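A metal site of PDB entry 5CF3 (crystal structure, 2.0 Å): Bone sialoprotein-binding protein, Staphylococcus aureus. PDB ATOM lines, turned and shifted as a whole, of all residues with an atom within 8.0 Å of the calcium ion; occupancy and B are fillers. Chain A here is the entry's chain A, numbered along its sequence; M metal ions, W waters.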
ATOM      1  N   ILE A  45      -0.439  17.726 -11.220  1.00  0.00           N
ATOM      2  CA  ILE A  45      -0.219  16.342 -11.612  1.00  0.00           C
ATOM      3  C   ILE A  45       0.151  15.530 -10.375  1.00  0.00           C
ATOM      4  O   ILE A  45       1.145  15.831  -9.723  1.00  0.00           O
ATOM      5  CB  ILE A  45       0.903  16.204 -12.674  1.00  0.00           C
ATOM      6  CG1 ILE A  45       0.625  17.108 -13.881  1.00  0.00           C
ATOM      7  CG2 ILE A  45       1.080  14.739 -13.072  1.00  0.00           C
ATOM      8  CD1 ILE A  45       1.754  17.158 -14.888  1.00  0.00           C
ATOM      9  N   ASP A  46      -0.634  14.498 -10.061  1.00  0.00           N
ATOM     10  CA  ASP A  46      -0.339  13.648  -8.902  1.00  0.00           C
ATOM     11  C   ASP A  46       1.001  12.968  -9.106  1.00  0.00           C
ATOM     12  O   ASP A  46       1.359  12.636 -10.243  1.00  0.00           O
ATOM     13  CB  ASP A  46      -1.451  12.622  -8.685  1.00  0.00           C
ATOM     14  CG  ASP A  46      -1.420  11.998  -7.298  1.00  0.00           C
ATOM     15  OD1 ASP A  46      -2.165  12.489  -6.409  1.00  0.00           O
ATOM     16  OD2 ASP A  46      -0.639  11.039  -7.091  1.00  0.00           O
ATOM     17  N   ASN A  47       1.729  12.743  -8.023  1.00  0.00           N
ATOM     18  CA  ASN A  47       2.989  12.000  -8.095  1.00  0.00           C
ATOM     19  C   ASN A  47       2.800  10.566  -8.639  1.00  0.00           C
ATOM     20  O   ASN A  47       3.716   9.971  -9.198  1.00  0.00           O
ATOM     21  CB  ASN A  47       3.675  11.986  -6.713  1.00  0.00           C
ATOM     22  CG  ASN A  47       4.167  13.368  -6.289  1.00  0.00           C
ATOM     23  OD1 ASN A  47       4.400  14.224  -7.140  1.00  0.00           O
ATOM     24  ND2 ASN A  47       4.301  13.598  -4.990  1.00  0.00           N
ATOM     25  N   ALA A  48       1.587  10.057  -8.492  1.00  0.00           N
ATOM     26  CA  ALA A  48       1.285   8.693  -8.901  1.00  0.00           C
ATOM     27  C   ALA A  48       1.299   8.543 -10.423  1.00  0.00           C
ATOM     28  O   ALA A  48       1.284   7.440 -10.942  1.00  0.00           O
ATOM     29  CB  ALA A  48      -0.065   8.268  -8.345  1.00  0.00           C
ATOM     30  N   VAL A  49       1.322   9.674 -11.128  1.00  0.00           N
ATOM     31  CA  VAL A  49       1.334   9.654 -12.581  1.00  0.00           C
ATOM     32  C   VAL A  49       2.728   9.244 -13.023  1.00  0.00           C
ATOM     33  O   VAL A  49       3.713   9.669 -12.429  1.00  0.00           O
ATOM     34  CB  VAL A  49       0.952  11.038 -13.191  1.00  0.00           C
ATOM     35  CG1 VAL A  49       1.194  11.068 -14.680  1.00  0.00           C
ATOM     36  CG2 VAL A  49      -0.487  11.365 -12.848  1.00  0.00           C
ATOM     37  N   LYS A  50       2.803   8.408 -14.056  1.00  0.00           N
ATOM     38  CA  LYS A  50       4.089   7.910 -14.499  1.00  0.00           C
ATOM     39  C   LYS A  50       4.213   8.031 -16.014  1.00  0.00           C
ATOM     40  O   LYS A  50       3.236   8.270 -16.698  1.00  0.00           O
ATOM     41  CB  LYS A  50       4.276   6.456 -14.084  1.00  0.00           C
ATOM     42  CG  LYS A  50       3.233   5.530 -14.668  1.00  0.00           C
ATOM     43  CD  LYS A  50       3.427   4.086 -14.247  1.00  0.00           C
ATOM     44  CE  LYS A  50       2.389   3.199 -14.921  1.00  0.00           C
ATOM     45  NZ  LYS A  50       0.986   3.634 -14.676  1.00  0.00           N
ATOM     46  N   ALA A  51       5.436   7.862 -16.502  1.00  0.00           N
ATOM     47  CA  ALA A  51       5.719   8.031 -17.921  1.00  0.00           C
ATOM     48  C   ALA A  51       4.858   7.072 -18.734  1.00  0.00           C
ATOM     49  O   ALA A  51       4.764   5.896 -18.405  1.00  0.00           O
ATOM     50  CB  ALA A  51       7.197   7.781 -18.200  1.00  0.00           C
ATOM     51  N   ASP A  53       1.609   7.367 -19.066  1.00  0.00           N
ATOM     52  CA  ASP A  53       0.206   7.631 -18.735  1.00  0.00           C
ATOM     53  C   ASP A  53      -0.340   8.696 -19.677  1.00  0.00           C
ATOM     54  O   ASP A  53       0.415   9.471 -20.275  1.00  0.00           O
ATOM     55  CB  ASP A  53       0.016   8.088 -17.290  1.00  0.00           C
ATOM     56  CG  ASP A  53       0.294   6.990 -16.265  1.00  0.00           C
ATOM     57  OD1 ASP A  53       0.494   7.355 -15.079  1.00  0.00           O
ATOM     58  OD2 ASP A  53       0.345   5.786 -16.617  1.00  0.00           O
ATOM     59  N   THR A 102       5.660  12.223 -20.694  1.00  0.00           N
ATOM     60  CA  THR A 102       7.055  11.846 -20.790  1.00  0.00           C
ATOM     61  C   THR A 102       7.594  11.440 -19.424  1.00  0.00           C
ATOM     62  O   THR A 102       6.857  11.459 -18.440  1.00  0.00           O
ATOM     63  CB  THR A 102       7.898  13.010 -21.332  1.00  0.00           C
ATOM     64  OG1 THR A 102       8.065  13.983 -20.289  1.00  0.00           O
ATOM     65  CG2 THR A 102       7.198  13.663 -22.524  1.00  0.00           C
ATOM     66  N   ASP A 103       8.888  11.137 -19.357  1.00  0.00           N
ATOM     67  CA  ASP A 103       9.497  10.715 -18.106  1.00  0.00           C
ATOM     68  C   ASP A 103       9.715  11.888 -17.143  1.00  0.00           C
ATOM     69  O   ASP A 103      10.236  11.701 -16.041  1.00  0.00           O
ATOM     70  CB  ASP A 103      10.804   9.967 -18.367  1.00  0.00           C
ATOM     71  CG  ASP A 103      11.880  10.844 -18.982  1.00  0.00           C
ATOM     72  OD1 ASP A 103      11.584  11.972 -19.440  1.00  0.00           O
ATOM     73  OD2 ASP A 103      13.044  10.400 -19.011  1.00  0.00           O
ATOM     74  N   TYR A 104       9.304  13.085 -17.559  1.00  0.00           N
ATOM     75  CA  TYR A 104       9.265  14.253 -16.688  1.00  0.00           C
ATOM     76  C   TYR A 104       8.560  13.898 -15.383  1.00  0.00           C
ATOM     77  O   TYR A 104       8.987  14.304 -14.311  1.00  0.00           O
ATOM     78  CB  TYR A 104       8.557  15.435 -17.361  1.00  0.00           C
ATOM     79  CG  TYR A 104       8.743  16.777 -16.671  1.00  0.00           C
ATOM     80  CD1 TYR A 104       7.923  17.160 -15.608  1.00  0.00           C
ATOM     81  CD2 TYR A 104       9.723  17.660 -17.091  1.00  0.00           C
ATOM     82  CE1 TYR A 104       8.097  18.394 -14.976  1.00  0.00           C
ATOM     83  CE2 TYR A 104       9.905  18.892 -16.480  1.00  0.00           C
ATOM     84  CZ  TYR A 104       9.092  19.254 -15.422  1.00  0.00           C
ATOM     85  OH  TYR A 104       9.281  20.474 -14.815  1.00  0.00           O
ATOM     86  N   VAL A 105       7.492  13.113 -15.486  1.00  0.00           N
ATOM     87  CA  VAL A 105       6.703  12.754 -14.307  1.00  0.00           C
ATOM     88  C   VAL A 105       7.325  11.592 -13.491  1.00  0.00           C
ATOM     89  O   VAL A 105       6.818  11.223 -12.416  1.00  0.00           O
ATOM     90  CB  VAL A 105       5.254  12.414 -14.709  1.00  0.00           C
ATOM     91  CG1 VAL A 105       4.562  13.670 -15.270  1.00  0.00           C
ATOM     92  CG2 VAL A 105       5.210  11.270 -15.724  1.00  0.00           C
ATOM     93  N   ASP A 106       8.435  11.042 -13.974  1.00  0.00           N
ATOM     94  CA  ASP A 106       9.225  10.105 -13.184  1.00  0.00           C
ATOM     95  C   ASP A 106      10.401  10.808 -12.507  1.00  0.00           C
ATOM     96  O   ASP A 106      10.901  10.372 -11.468  1.00  0.00           O
ATOM     97  CB  ASP A 106       9.760   8.957 -14.044  1.00  0.00           C
ATOM     98  CG  ASP A 106       8.661   8.024 -14.537  1.00  0.00           C
ATOM     99  OD1 ASP A 106       7.498   8.155 -14.098  1.00  0.00           O
ATOM    100  OD2 ASP A 106       8.966   7.155 -15.382  1.00  0.00           O
ATOM    101  N   ARG A 107      10.843  11.900 -13.127  1.00  0.00           N
ATOM    102  CA  ARG A 107      12.012  12.655 -12.679  1.00  0.00           C
ATOM    103  C   ARG A 107      11.673  13.737 -11.663  1.00  0.00           C
ATOM    104  O   ARG A 107      12.508  14.074 -10.831  1.00  0.00           O
ATOM    105  CB  ARG A 107      12.729  13.296 -13.876  1.00  0.00           C
ATOM    106  CG  ARG A 107      13.384  12.296 -14.820  1.00  0.00           C
ATOM    107  CD  ARG A 107      13.326  12.761 -16.274  1.00  0.00           C
ATOM    108  NE  ARG A 107      13.931  14.086 -16.457  1.00  0.00           N
ATOM    109  CZ  ARG A 107      13.545  14.956 -17.387  1.00  0.00           C
ATOM    110  NH1 ARG A 107      12.546  14.644 -18.210  1.00  0.00           N
ATOM    111  NH2 ARG A 107      14.143  16.129 -17.495  1.00  0.00           N
ATOM    112  N   TYR A 108      10.459  14.272 -11.720  1.00  0.00           N
ATOM    113  CA  TYR A 108      10.070  15.360 -10.822  1.00  0.00           C
ATOM    114  C   TYR A 108       8.770  15.045 -10.105  1.00  0.00           C
ATOM    115  O   TYR A 108       7.957  14.258 -10.587  1.00  0.00           O
ATOM    116  CB  TYR A 108       9.922  16.690 -11.583  1.00  0.00           C
ATOM    117  CG  TYR A 108      11.149  17.057 -12.375  1.00  0.00           C
ATOM    118  CD1 TYR A 108      11.143  16.994 -13.766  1.00  0.00           C
ATOM    119  CD2 TYR A 108      12.337  17.422 -11.741  1.00  0.00           C
ATOM    120  CE1 TYR A 108      12.260  17.300 -14.506  1.00  0.00           C
ATOM    121  CE2 TYR A 108      13.467  17.749 -12.469  1.00  0.00           C
ATOM    122  CZ  TYR A 108      13.426  17.678 -13.854  1.00  0.00           C
ATOM    123  OH  TYR A 108      14.550  17.994 -14.588  1.00  0.00           O
ATOM    124  N   GLU A 109       8.592  15.658  -8.943  1.00  0.00           N
ATOM    125  CA  GLU A 109       7.434  15.396  -8.104  1.00  0.00           C
ATOM    126  C   GLU A 109       6.775  16.706  -7.742  1.00  0.00           C
ATOM    127  O   GLU A 109       7.370  17.766  -7.942  1.00  0.00           O
ATOM    128  CB  GLU A 109       7.839  14.648  -6.838  1.00  0.00           C
ATOM    129  CG  GLU A 109       8.327  15.551  -5.726  1.00  0.00           C
ATOM    130  CD  GLU A 109       8.776  14.787  -4.498  1.00  0.00           C
ATOM    131  OE1 GLU A 109       9.577  13.843  -4.648  1.00  0.00           O
ATOM    132  OE2 GLU A 109       8.313  15.118  -3.388  1.00  0.00           O
ATOM    133  N   ASN A 110       5.579  16.623  -7.170  1.00  0.00           N
ATOM    134  CA  ASN A 110       4.777  17.793  -6.827  1.00  0.00           C
ATOM    135  C   ASN A 110       4.668  18.769  -7.991  1.00  0.00           C
ATOM    136  O   ASN A 110       4.868  19.975  -7.825  1.00  0.00           O
ATOM    137  CB  ASN A 110       5.354  18.478  -5.596  1.00  0.00           C
ATOM    138  CG  ASN A 110       5.492  17.521  -4.433  1.00  0.00           C
ATOM    139  OD1 ASN A 110       4.646  16.635  -4.254  1.00  0.00           O
ATOM    140  ND2 ASN A 110       6.569  17.653  -3.662  1.00  0.00           N
ATOM    141  N   VAL A 111       4.316  18.248  -9.158  1.00  0.00           N
ATOM    142  CA  VAL A 111       4.341  19.046 -10.357  1.00  0.00           C
ATOM    143  C   VAL A 111       2.975  19.639 -10.700  1.00  0.00           C
ATOM    144  O   VAL A 111       1.944  18.957 -10.700  1.00  0.00           O
ATOM    145  CB  VAL A 111       4.871  18.211 -11.542  1.00  0.00           C
ATOM    146  CG1 VAL A 111       4.655  18.936 -12.881  1.00  0.00           C
ATOM    147  CG2 VAL A 111       6.339  17.896 -11.292  1.00  0.00           C
HETATM  148 CA    CA M   1       5.358  10.308 -10.805  1.00  0.00          CA
HETATM  149  O   HOH W   1       3.946  12.342 -11.325  1.00  0.00           O
HETATM  150  O   HOH W   2       6.558   8.191 -11.556  1.00  0.00           O
HETATM  151  O   HOH W   3       6.608  12.114  -9.514  1.00  0.00           O
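Within 4 Å of the calcium ion: Asn 47, Val 49 and Val 105. The nearest printed residue that does not touch the calcium ion is Ala 48 (4.4 Å).
The side-chain amide oxygen of Asn 47 sits at hydrogen-bond distance from the backbone NH of Asn 110.
The calcium ion is bound by O of Asn 47. The backbone carbonyl oxygen (O) of Val 105 is bound to the calcium ion, at 2.4 Å. The backbone carbonyl oxygen (O) of Val 49 is bound to the calcium ion. Water W1 binds the calcium ion (2.5 Å). Water W2 is bound to the calcium ion (2.5 Å). The calcium ion is bound by water W3 (2.5 Å).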
